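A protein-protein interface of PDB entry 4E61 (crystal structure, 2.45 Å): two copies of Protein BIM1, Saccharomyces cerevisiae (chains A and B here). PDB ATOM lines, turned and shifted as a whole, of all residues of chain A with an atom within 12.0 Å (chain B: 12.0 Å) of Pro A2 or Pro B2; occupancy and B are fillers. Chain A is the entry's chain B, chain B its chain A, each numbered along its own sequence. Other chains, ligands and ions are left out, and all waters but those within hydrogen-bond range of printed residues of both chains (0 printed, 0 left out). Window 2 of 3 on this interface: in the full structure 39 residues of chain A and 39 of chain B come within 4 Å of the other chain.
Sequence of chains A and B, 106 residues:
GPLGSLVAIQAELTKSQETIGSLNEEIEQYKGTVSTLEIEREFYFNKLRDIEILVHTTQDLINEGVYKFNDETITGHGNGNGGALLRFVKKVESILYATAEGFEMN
The side-chain hydroxyl of Ser B5 is in hydrogen-bond range of the backbone carbonyl oxygen of Pro B2, 2.9 Å away.
Pro B2 touches Pro A2 (CB to CB, 3.8 Å). CD1 of Leu B6 touches CB of Ser A5, 3.9 Å away. Leu A6 touches Ser B5 (CD2 to OG, 3.4 Å). Leu A6 touches Leu B6. Ile B9 touches Leu A6 (CD1 to CD2, 3.8 Å). Leu B6 touches Ile A9 (CD1 to CD1, 3.5 Å). Ile A9 touches Ile B9 (CG2 to CG1, 3.3 Å). NE2 of Gln B10 touches CD1 of Ile A9, at 3.2 Å.
Pro A2 touches just one residue of chain B: Pro B2 (3.8 Å). Of chain A, only Pro A2 (3.8 Å) comes within 4 Å of Pro B2. Ser A5 touches just one residue of chain B: Leu B6 (3.9 Å). Leu A6 touches three residues of chain B. No residue of chain A comes within 4 Å of Gly B1. No residue of chain A comes within 4 Å of Leu B3. No residue of chain A comes within 4 Å of Gly B4. Of chain A, only Leu A6 comes within 4 Å of Ser B5. Leu B6 touches three residues of chain A. Of the printed residues of chain A, Ile B9 touches Leu A6 (3.8 Å) and Ile A9 (3.3 Å). Printed residues of chain B within 4 Å of Ile A9: Leu B6, Ile B9 and Gln B10. Printed residues of chain A within 4 Å of Gln B10: Ile A9. Ala A11 touches none of the printed residues of chain B. The nearest residue of chain B that does not touch Pro A2 is Leu B6 (5.2 Å). The nearest residue of chain A that does not touch Pro B2 is Leu A6 (4.3 Å). The nearest printed residue of chain B that does not touch Ile A9 is Ala B11 (6.2 Å).
Printed residues of chain A that touch a printed residue of chain B: Pro A2, Ser A5, Leu A6 and Ile A9. Along chain A the printed residues that touch a printed residue of chain B span positions 2 to 9. Hydrophobic or aromatic side chains of chain B within 4 Å of the printed part of chain A: Pro B2, Leu B6 and Ile B9. Among the printed residues, 8 pairs touch across the chains.
Pro A2 touches its own counterpart, Pro B2. Ser A5 touches Leu B6, and with the chains exchanged Leu A6 touches Ser B5. Leu A6 touches Ile B9, and with the chains exchanged Ile A9 touches Leu B6. Ile A9 touches its own counterpart, Ile B9. 11 positions are printed for both chains.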
ATOM      1  N   GLY A   1     -23.697   5.695   8.826  1.00  0.00           N
ATOM      2  CA  GLY A   1     -23.403   5.595   7.402  1.00  0.00           C
ATOM      3  C   GLY A   1     -23.777   6.868   6.666  1.00  0.00           C
ATOM      4  O   GLY A   1     -24.095   7.877   7.310  1.00  0.00           O
ATOM      5  N   PRO A   2     -23.788   6.841   5.310  1.00  0.00           N
ATOM      6  CA  PRO A   2     -24.145   8.057   4.539  1.00  0.00           C
ATOM      7  C   PRO A   2     -25.486   8.720   4.883  1.00  0.00           C
ATOM      8  O   PRO A   2     -25.565   9.937   5.009  1.00  0.00           O
ATOM      9  CB  PRO A   2     -24.097   7.575   3.067  1.00  0.00           C
ATOM     10  CG  PRO A   2     -24.181   6.075   3.133  1.00  0.00           C
ATOM     11  CD  PRO A   2     -23.492   5.700   4.417  1.00  0.00           C
ATOM     12  N   LEU A   3     -26.537   7.898   5.019  1.00  0.00           N
ATOM     13  CA  LEU A   3     -27.908   8.303   5.306  1.00  0.00           C
ATOM     14  C   LEU A   3     -28.024   8.984   6.646  1.00  0.00           C
ATOM     15  O   LEU A   3     -28.667  10.023   6.727  1.00  0.00           O
ATOM     16  CB  LEU A   3     -28.891   7.123   5.171  1.00  0.00           C
ATOM     17  CG  LEU A   3     -30.381   7.453   5.015  1.00  0.00           C
ATOM     18  CD1 LEU A   3     -30.639   8.423   3.882  1.00  0.00           C
ATOM     19  CD2 LEU A   3     -31.163   6.225   4.818  1.00  0.00           C
ATOM     20  N   GLY A   4     -27.370   8.423   7.658  1.00  0.00           N
ATOM     21  CA  GLY A   4     -27.365   8.957   9.012  1.00  0.00           C
ATOM     22  C   GLY A   4     -26.778  10.347   9.049  1.00  0.00           C
ATOM     23  O   GLY A   4     -27.390  11.245   9.638  1.00  0.00           O
ATOM     24  N   SER A   5     -25.614  10.549   8.370  1.00  0.00           N
ATOM     25  CA  SER A   5     -24.933  11.845   8.302  1.00  0.00           C
ATOM     26  C   SER A   5     -25.775  12.858   7.540  1.00  0.00           C
ATOM     27  O   SER A   5     -25.854  14.016   7.969  1.00  0.00           O
ATOM     28  CB  SER A   5     -23.542  11.718   7.685  1.00  0.00           C
ATOM     29  OG  SER A   5     -22.688  10.902   8.463  1.00  0.00           O
ATOM     30  N   LEU A   6     -26.448  12.413   6.447  1.00  0.00           N
ATOM     31  CA  LEU A   6     -27.332  13.263   5.644  1.00  0.00           C
ATOM     32  C   LEU A   6     -28.520  13.768   6.489  1.00  0.00           C
ATOM     33  O   LEU A   6     -28.877  14.952   6.427  1.00  0.00           O
ATOM     34  CB  LEU A   6     -27.841  12.511   4.400  1.00  0.00           C
ATOM     35  CG  LEU A   6     -26.898  12.414   3.198  1.00  0.00           C
ATOM     36  CD1 LEU A   6     -27.375  11.353   2.199  1.00  0.00           C
ATOM     37  CD2 LEU A   6     -26.748  13.739   2.505  1.00  0.00           C
ATOM     38  N   VAL A   7     -29.105  12.858   7.294  1.00  0.00           N
ATOM     39  CA  VAL A   7     -30.242  13.124   8.175  1.00  0.00           C
ATOM     40  C   VAL A   7     -29.823  14.103   9.296  1.00  0.00           C
ATOM     41  O   VAL A   7     -30.538  15.071   9.524  1.00  0.00           O
ATOM     42  CB  VAL A   7     -30.904  11.801   8.704  1.00  0.00           C
ATOM     43  CG1 VAL A   7     -31.871  12.069   9.855  1.00  0.00           C
ATOM     44  CG2 VAL A   7     -31.623  11.066   7.580  1.00  0.00           C
ATOM     45  N   ALA A   8     -28.678  13.860   9.972  1.00  0.00           N
ATOM     46  CA  ALA A   8     -28.176  14.724  11.043  1.00  0.00           C
ATOM     47  C   ALA A   8     -27.903  16.138  10.571  1.00  0.00           C
ATOM     48  O   ALA A   8     -28.255  17.070  11.286  1.00  0.00           O
ATOM     49  CB  ALA A   8     -26.924  14.136  11.668  1.00  0.00           C
ATOM     50  N   ILE A   9     -27.294  16.310   9.378  1.00  0.00           N
ATOM     51  CA  ILE A   9     -27.023  17.644   8.844  1.00  0.00           C
ATOM     52  C   ILE A   9     -28.294  18.331   8.455  1.00  0.00           C
ATOM     53  O   ILE A   9     -28.434  19.511   8.784  1.00  0.00           O
ATOM     54  CB  ILE A   9     -25.928  17.726   7.745  1.00  0.00           C
ATOM     55  CG1 ILE A   9     -24.568  17.373   8.339  1.00  0.00           C
ATOM     56  CG2 ILE A   9     -25.879  19.153   7.120  1.00  0.00           C
ATOM     57  CD1 ILE A   9     -23.570  17.161   7.310  1.00  0.00           C
ATOM     58  N   GLN A  10     -29.222  17.616   7.770  1.00  0.00           N
ATOM     59  CA  GLN A  10     -30.523  18.158   7.370  1.00  0.00           C
ATOM     60  C   GLN A  10     -31.329  18.696   8.590  1.00  0.00           C
ATOM     61  O   GLN A  10     -31.972  19.740   8.490  1.00  0.00           O
ATOM     62  CB  GLN A  10     -31.330  17.099   6.607  1.00  0.00           C
ATOM     63  CG  GLN A  10     -32.721  17.552   6.147  1.00  0.00           C
ATOM     64  CD  GLN A  10     -32.665  18.656   5.124  1.00  0.00           C
ATOM     65  OE1 GLN A  10     -32.855  19.836   5.434  1.00  0.00           O
ATOM     66  NE2 GLN A  10     -32.371  18.292   3.888  1.00  0.00           N
ATOM     67  N   ALA A  11     -31.249  18.006   9.727  1.00  0.00           N
ATOM     68  CA  ALA A  11     -31.921  18.376  10.967  1.00  0.00           C
ATOM     69  C   ALA A  11     -31.306  19.662  11.561  1.00  0.00           C
ATOM     70  O   ALA A  11     -32.041  20.586  11.937  1.00  0.00           O
ATOM     71  CB  ALA A  11     -31.826  17.228  11.965  1.00  0.00           C
ATOM     72  N   GLY B   1     -23.166  11.285  -5.907  1.00  0.00           N
ATOM     73  CA  GLY B   1     -23.839  10.339  -5.026  1.00  0.00           C
ATOM     74  C   GLY B   1     -23.990  10.840  -3.603  1.00  0.00           C
ATOM     75  O   GLY B   1     -24.084  12.054  -3.400  1.00  0.00           O
ATOM     76  N   PRO B   2     -24.024   9.933  -2.585  1.00  0.00           N
ATOM     77  CA  PRO B   2     -24.210  10.392  -1.187  1.00  0.00           C
ATOM     78  C   PRO B   2     -23.187  11.402  -0.679  1.00  0.00           C
ATOM     79  O   PRO B   2     -23.581  12.320   0.032  1.00  0.00           O
ATOM     80  CB  PRO B   2     -24.173   9.102  -0.367  1.00  0.00           C
ATOM     81  CG  PRO B   2     -24.514   8.049  -1.330  1.00  0.00           C
ATOM     82  CD  PRO B   2     -23.981   8.459  -2.660  1.00  0.00           C
ATOM     83  N   LEU B   3     -21.891  11.253  -1.039  1.00  0.00           N
ATOM     84  CA  LEU B   3     -20.817  12.160  -0.622  1.00  0.00           C
ATOM     85  C   LEU B   3     -21.010  13.588  -1.154  1.00  0.00           C
ATOM     86  O   LEU B   3     -20.840  14.545  -0.412  1.00  0.00           O
ATOM     87  CB  LEU B   3     -19.443  11.594  -1.027  1.00  0.00           C
ATOM     88  CG  LEU B   3     -18.165  12.126  -0.354  1.00  0.00           C
ATOM     89  CD1 LEU B   3     -17.645  13.411  -0.967  1.00  0.00           C
ATOM     90  CD2 LEU B   3     -18.296  12.239   1.105  1.00  0.00           C
ATOM     91  N   GLY B   4     -21.391  13.701  -2.414  1.00  0.00           N
ATOM     92  CA  GLY B   4     -21.668  14.979  -3.055  1.00  0.00           C
ATOM     93  C   GLY B   4     -22.795  15.729  -2.379  1.00  0.00           C
ATOM     94  O   GLY B   4     -22.658  16.919  -2.071  1.00  0.00           O
ATOM     95  N   SER B   5     -23.898  15.013  -2.100  1.00  0.00           N
ATOM     96  CA  SER B   5     -25.049  15.601  -1.420  1.00  0.00           C
ATOM     97  C   SER B   5     -24.723  15.965   0.053  1.00  0.00           C
ATOM     98  O   SER B   5     -25.161  17.004   0.524  1.00  0.00           O
ATOM     99  CB  SER B   5     -26.274  14.711  -1.563  1.00  0.00           C
ATOM    100  OG  SER B   5     -26.125  13.534  -0.804  1.00  0.00           O
ATOM    101  N   LEU B   6     -23.876  15.168   0.726  1.00  0.00           N
ATOM    102  CA  LEU B   6     -23.403  15.460   2.076  1.00  0.00           C
ATOM    103  C   LEU B   6     -22.564  16.745   2.100  1.00  0.00           C
ATOM    104  O   LEU B   6     -22.733  17.565   3.002  1.00  0.00           O
ATOM    105  CB  LEU B   6     -22.566  14.303   2.645  1.00  0.00           C
ATOM    106  CG  LEU B   6     -21.971  14.556   4.016  1.00  0.00           C
ATOM    107  CD1 LEU B   6     -23.049  14.530   5.072  1.00  0.00           C
ATOM    108  CD2 LEU B   6     -20.877  13.558   4.329  1.00  0.00           C
ATOM    109  N   VAL B   7     -21.668  16.915   1.098  1.00  0.00           N
ATOM    110  CA  VAL B   7     -20.814  18.090   0.940  1.00  0.00           C
ATOM    111  C   VAL B   7     -21.679  19.348   0.681  1.00  0.00           C
ATOM    112  O   VAL B   7     -21.480  20.354   1.358  1.00  0.00           O
ATOM    113  CB  VAL B   7     -19.700  17.842  -0.134  1.00  0.00           C
ATOM    114  CG1 VAL B   7     -19.011  19.140  -0.560  1.00  0.00           C
ATOM    115  CG2 VAL B   7     -18.668  16.819   0.362  1.00  0.00           C
ATOM    116  N   ALA B   8     -22.654  19.268  -0.254  1.00  0.00           N
ATOM    117  CA  ALA B   8     -23.549  20.389  -0.562  1.00  0.00           C
ATOM    118  C   ALA B   8     -24.402  20.823   0.645  1.00  0.00           C
ATOM    119  O   ALA B   8     -24.553  22.031   0.857  1.00  0.00           O
ATOM    120  CB  ALA B   8     -24.444  20.055  -1.733  1.00  0.00           C
ATOM    121  N   ILE B   9     -24.923  19.859   1.454  1.00  0.00           N
ATOM    122  CA  ILE B   9     -25.749  20.235   2.605  1.00  0.00           C
ATOM    123  C   ILE B   9     -24.938  20.741   3.802  1.00  0.00           C
ATOM    124  O   ILE B   9     -25.401  21.636   4.511  1.00  0.00           O
ATOM    125  CB  ILE B   9     -27.012  19.366   2.926  1.00  0.00           C
ATOM    126  CG1 ILE B   9     -26.872  18.394   4.087  1.00  0.00           C
ATOM    127  CG2 ILE B   9     -27.633  18.736   1.695  1.00  0.00           C
ATOM    128  CD1 ILE B   9     -26.014  17.196   3.892  1.00  0.00           C
ATOM    129  N   GLN B  10     -23.702  20.238   3.961  1.00  0.00           N
ATOM    130  CA  GLN B  10     -22.760  20.697   4.975  1.00  0.00           C
ATOM    131  C   GLN B  10     -22.343  22.156   4.692  1.00  0.00           C
ATOM    132  O   GLN B  10     -22.175  22.940   5.635  1.00  0.00           O
ATOM    133  CB  GLN B  10     -21.526  19.782   4.997  1.00  0.00           C
ATOM    134  CG  GLN B  10     -20.407  20.176   5.970  1.00  0.00           C
ATOM    135  CD  GLN B  10     -20.832  20.123   7.410  1.00  0.00           C
ATOM    136  OE1 GLN B  10     -21.116  21.158   8.029  1.00  0.00           O
ATOM    137  NE2 GLN B  10     -20.914  18.917   7.960  1.00  0.00           N
ATOM    138  N   ALA B  11     -22.178  22.506   3.398  1.00  0.00           N
ATOM    139  CA  ALA B  11     -21.824  23.842   2.942  1.00  0.00           C
ATOM    140  C   ALA B  11     -22.969  24.819   3.238  1.00  0.00           C
ATOM    141  O   ALA B  11     -22.709  25.903   3.742  1.00  0.00           O
ATOM    142  CB  ALA B  11     -21.492  23.828   1.463  1.00  0.00           C
ATOM    143  N   GLU B  12     -24.230  24.415   2.973  1.00  0.00           N
ATOM    144  CA  GLU B  12     -25.438  25.195   3.264  1.00  0.00           C
ATOM    145  C   GLU B  12     -25.543  25.446   4.770  1.00  0.00           C
ATOM    146  O   GLU B  12     -25.910  26.551   5.188  1.00  0.00           O
ATOM    147  CB  GLU B  12     -26.709  24.438   2.817  1.00  0.00           C
ATOM    148  CG  GLU B  12     -26.940  24.361   1.313  1.00  0.00           C
ATOM    149  CD  GLU B  12     -27.839  23.224   0.836  1.00  0.00           C
ATOM    150  OE1 GLU B  12     -28.981  23.106   1.339  1.00  0.00           O
ATOM    151  OE2 GLU B  12     -27.408  22.468  -0.068  1.00  0.00           O
